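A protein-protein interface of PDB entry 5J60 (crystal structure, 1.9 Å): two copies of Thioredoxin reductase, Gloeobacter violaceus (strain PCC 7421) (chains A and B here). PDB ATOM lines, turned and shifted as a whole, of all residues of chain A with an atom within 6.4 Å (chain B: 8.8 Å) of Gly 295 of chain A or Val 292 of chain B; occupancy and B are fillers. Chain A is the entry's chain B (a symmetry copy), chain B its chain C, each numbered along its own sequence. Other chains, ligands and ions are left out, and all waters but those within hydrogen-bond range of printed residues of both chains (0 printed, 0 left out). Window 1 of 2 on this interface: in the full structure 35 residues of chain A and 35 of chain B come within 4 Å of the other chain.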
ATOM      1  N   PRO A  18      13.104 -16.148  36.845  1.00  0.00           N
ATOM      2  CA  PRO A  18      13.747 -15.599  35.637  1.00  0.00           C
ATOM      3  C   PRO A  18      13.561 -16.463  34.407  1.00  0.00           C
ATOM      4  O   PRO A  18      13.510 -15.918  33.300  1.00  0.00           O
ATOM      5  CB  PRO A  18      15.230 -15.473  36.025  1.00  0.00           C
ATOM      6  CG  PRO A  18      15.415 -16.483  37.182  1.00  0.00           C
ATOM      7  CD  PRO A  18      14.080 -16.482  37.908  1.00  0.00           C
ATOM      8  N   ALA A  19      13.467 -17.786  34.543  1.00  0.00           N
ATOM      9  CA  ALA A  19      13.221 -18.595  33.357  1.00  0.00           C
ATOM     10  C   ALA A  19      11.842 -18.295  32.782  1.00  0.00           C
ATOM     11  O   ALA A  19      11.717 -17.962  31.593  1.00  0.00           O
ATOM     12  CB  ALA A  19      13.366 -20.079  33.651  1.00  0.00           C
ATOM     13  N   THR A  22      11.447 -14.654  31.394  1.00  0.00           N
ATOM     14  CA  THR A  22      12.111 -14.463  30.114  1.00  0.00           C
ATOM     15  C   THR A  22      11.357 -15.174  29.001  1.00  0.00           C
ATOM     16  O   THR A  22      11.223 -14.634  27.895  1.00  0.00           O
ATOM     17  CB  THR A  22      13.555 -14.964  30.153  1.00  0.00           C
ATOM     18  OG1 THR A  22      14.310 -14.245  31.121  1.00  0.00           O
ATOM     19  CG2 THR A  22      14.213 -14.780  28.764  1.00  0.00           C
ATOM     20  N   MET A 269      14.778 -27.317  24.524  1.00  0.00           N
ATOM     21  CA  MET A 269      14.130 -27.279  25.829  1.00  0.00           C
ATOM     22  C   MET A 269      12.796 -28.021  25.848  1.00  0.00           C
ATOM     23  O   MET A 269      12.035 -27.893  26.827  1.00  0.00           O
ATOM     24  CB  MET A 269      13.919 -25.845  26.322  1.00  0.00           C
ATOM     25  CG  MET A 269      15.217 -25.007  26.401  1.00  0.00           C
ATOM     26  SD  MET A 269      16.349 -25.678  27.656  1.00  0.00           S
ATOM     27  CE  MET A 269      17.962 -25.192  27.004  1.00  0.00           C
ATOM     28  N   ALA A 290      21.044 -17.314  37.388  1.00  0.00           N
ATOM     29  CA  ALA A 290      19.868 -16.626  36.862  1.00  0.00           C
ATOM     30  C   ALA A 290      19.964 -16.415  35.351  1.00  0.00           C
ATOM     31  O   ALA A 290      18.969 -16.573  34.632  1.00  0.00           O
ATOM     32  CB  ALA A 290      19.691 -15.299  37.599  1.00  0.00           C
ATOM     33  N   VAL A 291      21.147 -16.063  34.841  1.00  0.00           N
ATOM     34  CA  VAL A 291      21.262 -15.805  33.408  1.00  0.00           C
ATOM     35  C   VAL A 291      21.134 -17.093  32.594  1.00  0.00           C
ATOM     36  O   VAL A 291      20.644 -17.065  31.460  1.00  0.00           O
ATOM     37  CB  VAL A 291      22.579 -15.070  33.089  1.00  0.00           C
ATOM     38  CG1 VAL A 291      23.788 -15.966  33.301  1.00  0.00           C
ATOM     39  CG2 VAL A 291      22.546 -14.554  31.672  1.00  0.00           C
ATOM     40  N   VAL A 292      21.533 -18.234  33.152  1.00  0.00           N
ATOM     41  CA  VAL A 292      21.344 -19.502  32.452  1.00  0.00           C
ATOM     42  C   VAL A 292      19.864 -19.847  32.395  1.00  0.00           C
ATOM     43  O   VAL A 292      19.344 -20.245  31.344  1.00  0.00           O
ATOM     44  CB  VAL A 292      22.176 -20.613  33.130  1.00  0.00           C
ATOM     45  CG1 VAL A 292      21.901 -21.981  32.458  1.00  0.00           C
ATOM     46  CG2 VAL A 292      23.663 -20.268  33.076  1.00  0.00           C
ATOM     47  N   ALA A 293      19.151 -19.667  33.512  1.00  0.00           N
ATOM     48  CA  ALA A 293      17.713 -19.889  33.533  1.00  0.00           C
ATOM     49  C   ALA A 293      16.998 -18.999  32.521  1.00  0.00           C
ATOM     50  O   ALA A 293      16.101 -19.460  31.804  1.00  0.00           O
ATOM     51  CB  ALA A 293      17.161 -19.655  34.943  1.00  0.00           C
ATOM     52  N   ALA A 294      17.387 -17.715  32.452  1.00  0.00           N
ATOM     53  CA  ALA A 294      16.818 -16.791  31.473  1.00  0.00           C
ATOM     54  C   ALA A 294      17.091 -17.254  30.043  1.00  0.00           C
ATOM     55  O   ALA A 294      16.191 -17.253  29.199  1.00  0.00           O
ATOM     56  CB  ALA A 294      17.380 -15.385  31.723  1.00  0.00           C
ATOM     57  N   GLY A 295      18.315 -17.698  29.766  1.00  0.00           N
ATOM     58  CA  GLY A 295      18.630 -18.227  28.447  1.00  0.00           C
ATOM     59  C   GLY A 295      17.764 -19.406  28.052  1.00  0.00           C
ATOM     60  O   GLY A 295      17.325 -19.511  26.893  1.00  0.00           O
ATOM     61  N   ASP A 296      17.524 -20.325  28.993  1.00  0.00           N
ATOM     62  CA  ASP A 296      16.610 -21.440  28.745  1.00  0.00           C
ATOM     63  C   ASP A 296      15.232 -20.943  28.307  1.00  0.00           C
ATOM     64  O   ASP A 296      14.626 -21.476  27.373  1.00  0.00           O
ATOM     65  CB  ASP A 296      16.417 -22.289  29.996  1.00  0.00           C
ATOM     66  CG  ASP A 296      17.525 -23.253  30.269  1.00  0.00           C
ATOM     67  OD1 ASP A 296      18.556 -23.219  29.581  1.00  0.00           O
ATOM     68  OD2 ASP A 296      17.354 -24.031  31.252  1.00  0.00           O
ATOM     69  N   GLY A 297      14.684 -19.980  29.046  1.00  0.00           N
ATOM     70  CA  GLY A 297      13.359 -19.469  28.730  1.00  0.00           C
ATOM     71  C   GLY A 297      13.294 -18.847  27.345  1.00  0.00           C
ATOM     72  O   GLY A 297      12.297 -18.996  26.627  1.00  0.00           O
ATOM     73  N   CYS A 298      14.360 -18.152  26.956  1.00  0.00           N
ATOM     74  CA  CYS A 298      14.432 -17.584  25.615  1.00  0.00           C
ATOM     75  C   CYS A 298      14.403 -18.677  24.554  1.00  0.00           C
ATOM     76  O   CYS A 298      13.630 -18.603  23.594  1.00  0.00           O
ATOM     77  CB  CYS A 298      15.692 -16.732  25.484  1.00  0.00           C
ATOM     78  SG  CYS A 298      15.943 -16.047  23.868  1.00  0.00           S
ATOM     79  N   ILE A 299      15.240 -19.704  24.712  1.00  0.00           N
ATOM     80  CA  ILE A 299      15.266 -20.805  23.747  1.00  0.00           C
ATOM     81  C   ILE A 299      13.886 -21.430  23.632  1.00  0.00           C
ATOM     82  O   ILE A 299      13.378 -21.663  22.527  1.00  0.00           O
ATOM     83  CB  ILE A 299      16.334 -21.845  24.139  1.00  0.00           C
ATOM     84  CG1 ILE A 299      17.746 -21.246  23.986  1.00  0.00           C
ATOM     85  CG2 ILE A 299      16.185 -23.112  23.275  1.00  0.00           C
ATOM     86  CD1 ILE A 299      18.872 -22.161  24.497  1.00  0.00           C
ATOM     87  N   ALA A 300      13.267 -21.745  24.780  1.00  0.00           N
ATOM     88  CA  ALA A 300      11.939 -22.344  24.747  1.00  0.00           C
ATOM     89  C   ALA A 300      10.948 -21.451  24.012  1.00  0.00           C
ATOM     90  O   ALA A 300      10.167 -21.937  23.187  1.00  0.00           O
ATOM     91  CB  ALA A 300      11.454 -22.651  26.164  1.00  0.00           C
ATOM     92  N   MET A 302      11.461 -19.294  21.661  1.00  0.00           N
ATOM     93  CA  MET A 302      11.739 -19.297  20.221  1.00  0.00           C
ATOM     94  C   MET A 302      11.294 -20.612  19.575  1.00  0.00           C
ATOM     95  O   MET A 302      10.741 -20.634  18.458  1.00  0.00           O
ATOM     96  CB  MET A 302      13.228 -19.037  20.005  1.00  0.00           C
ATOM     97  CG  MET A 302      13.662 -17.651  20.468  1.00  0.00           C
ATOM     98  SD  MET A 302      15.436 -17.400  20.320  1.00  0.00           S
ATOM     99  CE  MET A 302      15.634 -17.092  18.574  1.00  0.00           C
ATOM    100  N   PRO B  18      28.699 -10.397  24.357  1.00  0.00           N
ATOM    101  CA  PRO B  18      28.049 -10.830  25.611  1.00  0.00           C
ATOM    102  C   PRO B  18      28.469 -12.230  26.058  1.00  0.00           C
ATOM    103  O   PRO B  18      28.518 -12.497  27.265  1.00  0.00           O
ATOM    104  CB  PRO B  18      26.554 -10.767  25.274  1.00  0.00           C
ATOM    105  CG  PRO B  18      26.498 -10.872  23.762  1.00  0.00           C
ATOM    106  CD  PRO B  18      27.731 -10.204  23.260  1.00  0.00           C
ATOM    107  N   ALA B  19      28.765 -13.138  25.129  1.00  0.00           N
ATOM    108  CA  ALA B  19      29.216 -14.466  25.538  1.00  0.00           C
ATOM    109  C   ALA B  19      30.563 -14.375  26.227  1.00  0.00           C
ATOM    110  O   ALA B  19      30.727 -14.835  27.363  1.00  0.00           O
ATOM    111  CB  ALA B  19      29.285 -15.401  24.333  1.00  0.00           C
ATOM    112  N   THR B  22      30.424 -12.383  29.578  1.00  0.00           N
ATOM    113  CA  THR B  22      29.811 -13.106  30.686  1.00  0.00           C
ATOM    114  C   THR B  22      30.740 -14.204  31.174  1.00  0.00           C
ATOM    115  O   THR B  22      30.869 -14.440  32.381  1.00  0.00           O
ATOM    116  CB  THR B  22      28.453 -13.679  30.278  1.00  0.00           C
ATOM    117  OG1 THR B  22      27.554 -12.618  29.905  1.00  0.00           O
ATOM    118  CG2 THR B  22      27.834 -14.459  31.430  1.00  0.00           C
ATOM    119  N   ASN B  54      14.737  -6.706  24.478  1.00  0.00           N
ATOM    120  CA  ASN B  54      14.356  -8.035  24.939  1.00  0.00           C
ATOM    121  C   ASN B  54      15.485  -8.686  25.712  1.00  0.00           C
ATOM    122  O   ASN B  54      15.553  -9.914  25.807  1.00  0.00           O
ATOM    123  CB  ASN B  54      13.914  -8.920  23.781  1.00  0.00           C
ATOM    124  CG  ASN B  54      14.930  -8.983  22.691  1.00  0.00           C
ATOM    125  OD1 ASN B  54      16.069  -8.522  22.854  1.00  0.00           O
ATOM    126  ND2 ASN B  54      14.528  -9.542  21.538  1.00  0.00           N
ATOM    127  N   TYR B  55      16.370  -7.885  26.309  1.00  0.00           N
ATOM    128  CA  TYR B  55      17.347  -8.445  27.229  1.00  0.00           C
ATOM    129  C   TYR B  55      16.722  -8.452  28.624  1.00  0.00           C
ATOM    130  O   TYR B  55      16.429  -7.372  29.167  1.00  0.00           O
ATOM    131  CB  TYR B  55      18.656  -7.655  27.210  1.00  0.00           C
ATOM    132  CG  TYR B  55      19.690  -8.401  27.983  1.00  0.00           C
ATOM    133  CD1 TYR B  55      20.401  -9.441  27.401  1.00  0.00           C
ATOM    134  CD2 TYR B  55      19.909  -8.134  29.317  1.00  0.00           C
ATOM    135  CE1 TYR B  55      21.313 -10.144  28.098  1.00  0.00           C
ATOM    136  CE2 TYR B  55      20.843  -8.845  30.030  1.00  0.00           C
ATOM    137  CZ  TYR B  55      21.534  -9.856  29.421  1.00  0.00           C
ATOM    138  OH  TYR B  55      22.468 -10.582  30.129  1.00  0.00           O
ATOM    139  N   PRO B  56      16.447  -9.616  29.218  1.00  0.00           N
ATOM    140  CA  PRO B  56      15.680  -9.642  30.473  1.00  0.00           C
ATOM    141  C   PRO B  56      16.465  -9.002  31.607  1.00  0.00           C
ATOM    142  O   PRO B  56      17.644  -9.287  31.789  1.00  0.00           O
ATOM    143  CB  PRO B  56      15.444 -11.139  30.726  1.00  0.00           C
ATOM    144  CG  PRO B  56      16.419 -11.842  29.907  1.00  0.00           C
ATOM    145  CD  PRO B  56      16.746 -10.978  28.734  1.00  0.00           C
ATOM    146  N   MET B  71      28.429  -5.014  30.576  1.00  0.00           N
ATOM    147  CA  MET B  71      28.968  -6.362  30.747  1.00  0.00           C
ATOM    148  C   MET B  71      30.490  -6.343  30.772  1.00  0.00           C
ATOM    149  O   MET B  71      31.125  -6.963  31.638  1.00  0.00           O
ATOM    150  CB  MET B  71      28.463  -7.263  29.616  1.00  0.00           C
ATOM    151  CG  MET B  71      26.970  -7.420  29.583  1.00  0.00           C
ATOM    152  SD  MET B  71      26.547  -8.459  28.162  1.00  0.00           S
ATOM    153  CE  MET B  71      24.774  -8.668  28.371  1.00  0.00           C
ATOM    154  N   MET B 269      29.554 -26.910  26.786  1.00  0.00           N
ATOM    155  CA  MET B 269      30.129 -25.966  25.828  1.00  0.00           C
ATOM    156  C   MET B 269      31.574 -26.314  25.465  1.00  0.00           C
ATOM    157  O   MET B 269      32.288 -25.476  24.920  1.00  0.00           O
ATOM    158  CB  MET B 269      30.069 -24.521  26.329  1.00  0.00           C
ATOM    159  CG  MET B 269      28.660 -24.051  26.717  1.00  0.00           C
ATOM    160  SD  MET B 269      27.530 -24.008  25.302  1.00  0.00           S
ATOM    161  CE  MET B 269      25.954 -24.361  26.097  1.00  0.00           C
ATOM    162  N   ILE B 279      31.254 -20.757  22.692  1.00  0.00           N
ATOM    163  CA  ILE B 279      30.091 -20.119  23.288  1.00  0.00           C
ATOM    164  C   ILE B 279      29.548 -19.039  22.364  1.00  0.00           C
ATOM    165  O   ILE B 279      30.295 -18.403  21.616  1.00  0.00           O
ATOM    166  CB  ILE B 279      30.417 -19.491  24.648  1.00  0.00           C
ATOM    167  CG1 ILE B 279      31.547 -18.448  24.489  1.00  0.00           C
ATOM    168  CG2 ILE B 279      30.734 -20.559  25.630  1.00  0.00           C
ATOM    169  CD1 ILE B 279      31.848 -17.663  25.748  1.00  0.00           C
ATOM    170  N   GLY B 280      28.240 -18.800  22.458  1.00  0.00           N
ATOM    171  CA  GLY B 280      27.647 -17.719  21.694  1.00  0.00           C
ATOM    172  C   GLY B 280      27.459 -18.120  20.239  1.00  0.00           C
ATOM    173  O   GLY B 280      27.386 -19.304  19.901  1.00  0.00           O
ATOM    174  N   ASP B 281      27.386 -17.120  19.364  1.00  0.00           N
ATOM    175  CA  ASP B 281      26.943 -17.381  17.998  1.00  0.00           C
ATOM    176  C   ASP B 281      28.012 -18.004  17.102  1.00  0.00           C
ATOM    177  O   ASP B 281      27.682 -18.414  15.984  1.00  0.00           O
ATOM    178  CB  ASP B 281      26.382 -16.093  17.395  1.00  0.00           C
ATOM    179  CG  ASP B 281      24.975 -15.811  17.900  1.00  0.00           C
ATOM    180  OD1 ASP B 281      24.393 -16.736  18.520  1.00  0.00           O
ATOM    181  OD2 ASP B 281      24.436 -14.709  17.687  1.00  0.00           O
ATOM    182  N   ARG B 283      28.854 -20.858  17.637  1.00  0.00           N
ATOM    183  CA  ARG B 283      28.258 -22.190  17.563  1.00  0.00           C
ATOM    184  C   ARG B 283      27.225 -22.286  16.456  1.00  0.00           C
ATOM    185  O   ARG B 283      26.837 -23.398  16.078  1.00  0.00           O
ATOM    186  CB  ARG B 283      27.571 -22.527  18.884  1.00  0.00           C
ATOM    187  CG  ARG B 283      28.467 -22.601  20.119  1.00  0.00           C
ATOM    188  CD  ARG B 283      27.628 -22.880  21.397  1.00  0.00           C
ATOM    189  NE  ARG B 283      26.719 -23.993  21.236  1.00  0.00           N
ATOM    190  CZ  ARG B 283      25.538 -24.115  21.822  1.00  0.00           C
ATOM    191  NH1 ARG B 283      25.061 -23.183  22.638  1.00  0.00           N
ATOM    192  NH2 ARG B 283      24.837 -25.199  21.588  1.00  0.00           N
ATOM    193  N   THR B 285      24.004 -21.829  16.434  1.00  0.00           N
ATOM    194  CA  THR B 285      22.688 -22.391  16.682  1.00  0.00           C
ATOM    195  C   THR B 285      21.652 -21.406  16.158  1.00  0.00           C
ATOM    196  O   THR B 285      21.965 -20.252  15.853  1.00  0.00           O
ATOM    197  CB  THR B 285      22.446 -22.651  18.169  1.00  0.00           C
ATOM    198  OG1 THR B 285      22.051 -21.421  18.782  1.00  0.00           O
ATOM    199  CG2 THR B 285      23.675 -23.239  18.897  1.00  0.00           C
ATOM    200  N   PRO B 286      20.401 -21.838  16.015  1.00  0.00           N
ATOM    201  CA  PRO B 286      19.351 -20.900  15.598  1.00  0.00           C
ATOM    202  C   PRO B 286      18.975 -19.893  16.667  1.00  0.00           C
ATOM    203  O   PRO B 286      18.328 -18.891  16.350  1.00  0.00           O
ATOM    204  CB  PRO B 286      18.173 -21.817  15.256  1.00  0.00           C
ATOM    205  CG  PRO B 286      18.467 -23.103  15.855  1.00  0.00           C
ATOM    206  CD  PRO B 286      19.924 -23.233  16.041  1.00  0.00           C
ATOM    207  N   PHE B 287      19.420 -20.081  17.903  1.00  0.00           N
ATOM    208  CA  PHE B 287      18.953 -19.261  19.019  1.00  0.00           C
ATOM    209  C   PHE B 287      19.920 -18.108  19.263  1.00  0.00           C
ATOM    210  O   PHE B 287      20.673 -18.052  20.246  1.00  0.00           O
ATOM    211  CB  PHE B 287      18.766 -20.144  20.250  1.00  0.00           C
ATOM    212  CG  PHE B 287      17.899 -21.344  19.987  1.00  0.00           C
ATOM    213  CD1 PHE B 287      16.536 -21.184  19.813  1.00  0.00           C
ATOM    214  CD2 PHE B 287      18.432 -22.614  19.905  1.00  0.00           C
ATOM    215  CE1 PHE B 287      15.716 -22.267  19.575  1.00  0.00           C
ATOM    216  CE2 PHE B 287      17.612 -23.722  19.651  1.00  0.00           C
ATOM    217  CZ  PHE B 287      16.265 -23.546  19.485  1.00  0.00           C
ATOM    218  N   LYS B 288      19.856 -17.145  18.346  1.00  0.00           N
ATOM    219  CA  LYS B 288      20.804 -16.033  18.293  1.00  0.00           C
ATOM    220  C   LYS B 288      20.208 -14.833  19.026  1.00  0.00           C
ATOM    221  O   LYS B 288      19.550 -13.976  18.432  1.00  0.00           O
ATOM    222  CB  LYS B 288      21.158 -15.701  16.842  1.00  0.00           C
ATOM    223  CG  LYS B 288      21.970 -16.822  16.147  1.00  0.00           C
ATOM    224  CD  LYS B 288      22.639 -16.328  14.867  1.00  0.00           C
ATOM    225  CE  LYS B 288      23.598 -17.368  14.312  1.00  0.00           C
ATOM    226  NZ  LYS B 288      22.826 -18.564  13.826  1.00  0.00           N
ATOM    227  N   GLN B 289      20.392 -14.814  20.341  1.00  0.00           N
ATOM    228  CA  GLN B 289      19.928 -13.731  21.196  1.00  0.00           C
ATOM    229  C   GLN B 289      21.012 -13.464  22.234  1.00  0.00           C
ATOM    230  O   GLN B 289      21.764 -14.371  22.600  1.00  0.00           O
ATOM    231  CB  GLN B 289      18.614 -14.066  21.915  1.00  0.00           C
ATOM    232  CG  GLN B 289      17.464 -14.524  21.021  1.00  0.00           C
ATOM    233  CD  GLN B 289      16.933 -13.437  20.139  1.00  0.00           C
ATOM    234  OE1 GLN B 289      16.943 -12.232  20.473  1.00  0.00           O
ATOM    235  NE2 GLN B 289      16.460 -13.847  18.988  1.00  0.00           N
ATOM    236  N   ALA B 290      21.089 -12.209  22.700  1.00  0.00           N
ATOM    237  CA  ALA B 290      22.144 -11.818  23.639  1.00  0.00           C
ATOM    238  C   ALA B 290      22.076 -12.619  24.936  1.00  0.00           C
ATOM    239  O   ALA B 290      23.115 -13.045  25.465  1.00  0.00           O
ATOM    240  CB  ALA B 290      22.053 -10.315  23.926  1.00  0.00           C
ATOM    241  N   VAL B 291      20.870 -12.850  25.472  1.00  0.00           N
ATOM    242  CA  VAL B 291      20.807 -13.553  26.753  1.00  0.00           C
ATOM    243  C   VAL B 291      21.206 -15.030  26.587  1.00  0.00           C
ATOM    244  O   VAL B 291      21.743 -15.639  27.517  1.00  0.00           O
ATOM    245  CB  VAL B 291      19.419 -13.405  27.397  1.00  0.00           C
ATOM    246  CG1 VAL B 291      18.319 -14.185  26.620  1.00  0.00           C
ATOM    247  CG2 VAL B 291      19.479 -13.862  28.837  1.00  0.00           C
ATOM    248  N   VAL B 292      20.967 -15.614  25.414  1.00  0.00           N
ATOM    249  CA  VAL B 292      21.377 -16.995  25.166  1.00  0.00           C
ATOM    250  C   VAL B 292      22.898 -17.080  25.086  1.00  0.00           C
ATOM    251  O   VAL B 292      23.522 -17.981  25.665  1.00  0.00           O
ATOM    252  CB  VAL B 292      20.699 -17.533  23.884  1.00  0.00           C
ATOM    253  CG1 VAL B 292      21.189 -18.944  23.552  1.00  0.00           C
ATOM    254  CG2 VAL B 292      19.185 -17.566  24.037  1.00  0.00           C
ATOM    255  N   ALA B 293      23.512 -16.142  24.358  1.00  0.00           N
ATOM    256  CA  ALA B 293      24.965 -16.056  24.293  1.00  0.00           C
ATOM    257  C   ALA B 293      25.570 -15.864  25.674  1.00  0.00           C
ATOM    258  O   ALA B 293      26.558 -16.526  26.023  1.00  0.00           O
ATOM    259  CB  ALA B 293      25.380 -14.897  23.383  1.00  0.00           C
ATOM    260  N   ALA B 294      24.986 -14.968  26.478  1.00  0.00           N
ATOM    261  CA  ALA B 294      25.463 -14.780  27.848  1.00  0.00           C
ATOM    262  C   ALA B 294      25.352 -16.075  28.649  1.00  0.00           C
ATOM    263  O   ALA B 294      26.290 -16.458  29.366  1.00  0.00           O
ATOM    264  CB  ALA B 294      24.680 -13.648  28.512  1.00  0.00           C
ATOM    265  N   GLY B 295      24.230 -16.788  28.511  1.00  0.00           N
ATOM    266  CA  GLY B 295      24.078 -18.055  29.213  1.00  0.00           C
ATOM    267  C   GLY B 295      25.137 -19.079  28.836  1.00  0.00           C
ATOM    268  O   GLY B 295      25.656 -19.791  29.703  1.00  0.00           O
ATOM    269  N   ASP B 296      25.451 -19.189  27.532  1.00  0.00           N
ATOM    270  CA  ASP B 296      26.556 -20.039  27.080  1.00  0.00           C
ATOM    271  C   ASP B 296      27.842 -19.690  27.828  1.00  0.00           C
ATOM    272  O   ASP B 296      28.572 -20.571  28.298  1.00  0.00           O
ATOM    273  CB  ASP B 296      26.808 -19.847  25.572  1.00  0.00           C
ATOM    274  CG  ASP B 296      25.866 -20.627  24.671  1.00  0.00           C
ATOM    275  OD1 ASP B 296      24.899 -21.251  25.166  1.00  0.00           O
ATOM    276  OD2 ASP B 296      26.112 -20.592  23.425  1.00  0.00           O
ATOM    277  N   GLY B 297      28.156 -18.399  27.895  1.00  0.00           N
ATOM    278  CA  GLY B 297      29.390 -17.968  28.541  1.00  0.00           C
ATOM    279  C   GLY B 297      29.440 -18.335  30.010  1.00  0.00           C
ATOM    280  O   GLY B 297      30.487 -18.742  30.526  1.00  0.00           O
ATOM    281  N   CYS B 298      28.303 -18.232  30.694  1.00  0.00           N
ATOM    282  CA  CYS B 298      28.233 -18.657  32.088  1.00  0.00           C
ATOM    283  C   CYS B 298      28.491 -20.162  32.230  1.00  0.00           C
ATOM    284  O   CYS B 298      29.295 -20.590  33.066  1.00  0.00           O
ATOM    285  CB  CYS B 298      26.871 -18.274  32.656  1.00  0.00           C
ATOM    286  SG  CYS B 298      26.652 -18.776  34.338  1.00  0.00           S
ATOM    287  N   ILE B 299      27.819 -20.982  31.424  1.00  0.00           N
ATOM    288  CA  ILE B 299      28.035 -22.431  31.491  1.00  0.00           C
ATOM    289  C   ILE B 299      29.510 -22.761  31.285  1.00  0.00           C
ATOM    290  O   ILE B 299      30.120 -23.495  32.074  1.00  0.00           O
ATOM    291  CB  ILE B 299      27.151 -23.154  30.457  1.00  0.00           C
ATOM    292  CG1 ILE B 299      25.662 -23.037  30.850  1.00  0.00           C
ATOM    293  CG2 ILE B 299      27.595 -24.637  30.310  1.00  0.00           C
ATOM    294  CD1 ILE B 299      24.677 -23.601  29.843  1.00  0.00           C
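Hydrophobic or aromatic side chains of chain B within 4 Å of the printed part of chain A: Pro 56, Phe 287, Val 291, Val 292 and Ala 294.
The side-chain hydroxyl of Thr 285 of chain B sits at hydrogen-bond distance from the backbone NH of Phe 287 of chain B (3.1 Å).
The backbone carbonyl oxygen (O) of Pro 18 of chain A lies within hydrogen-bond range of the side-chain hydroxyl (OG1) of Thr 22 of chain A (2.9 Å).
Ala 290 of chain A touches none of the printed residues of chain B.
Printed residues of chain B within 4 Å of Val 292 of chain A: Gly 295 and Cys 298.
Ala 294 of chain A touches just one residue of chain B: Val 291.
Lys 288 of chain B touches none of the printed residues of chain A.
Of the printed residues of chain A, Gln 289 of chain B touches Cys 298 and Met 302.
Val 292 of chain B touches just these residues of chain A: Gly 295 (3.9 Å), Cys 298 (3.6 Å) and Ile 299 (3.95 Å).
Printed residues of chain A within 4 Å of Cys 298 of chain B: Val 291 (3.9 Å) and Val 292 (3.6 Å).
The nearest residue of chain B that does not touch Gly 295 of chain A is Val 291 of chain B (4.1 Å).
The nearest printed residue of chain A that does not touch Pro 286 of chain B is Ile 299 of chain A (7.5 Å).
Among the printed residues, merely in contact across the chains: Thr 22 of chain A with Pro 56 of chain B (3.3 Å), Met 302 of chain A with Gln 289 of chain B (3.4 Å), Cys 298 of chain A with Gln 289 of chain B (3.6 Å), Val 292 of chain A with Cys 298 of chain B (3.6 Å), Cys 298 of chain A with Val 292 of chain B (3.6 Å), Ile 299 of chain A with Phe 287 of chain B (3.8 Å), Cys 298 of chain A with Val 291 of chain B (3.8 Å), Ala 294 of chain A with Val 291 of chain B (3.9 Å), Val 291 of chain A with Cys 298 of chain B (3.9 Å), Val 291 of chain A with Ala 294 of chain B (3.9 Å), Gly 295 of chain A with Val 292 of chain B (3.9 Å), Met 302 of chain A with Pro 286 of chain B (3.9 Å), Val 292 of chain A with Gly 295 of chain B (3.9 Å), Met 302 of chain A with Phe 287 of chain B (3.9 Å) and Ile 299 of chain A with Val 292 of chain B (3.95 Å).
Val 291 of chain A touches Cys 298 of chain B, and with the chains exchanged Cys 298 of chain A touches Val 291 of chain B.
Val 292 of chain A touches Gly 295 of chain B, and with the chains exchanged Gly 295 of chain A touches Val 292 of chain B.
Val 292 of chain A touches Cys 298 of chain B, and with the chains exchanged Cys 298 of chain A touches Val 292 of chain B.
Ile 299 of chain A touches Val 292 of chain B, but with the chains exchanged Val 292 of chain A does not touch Ile 299 of chain B (4.1 Å).
Of the 15 pairs that touch across the chains among the printed residues, 8 have their exchanged pair printed and touching as well.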
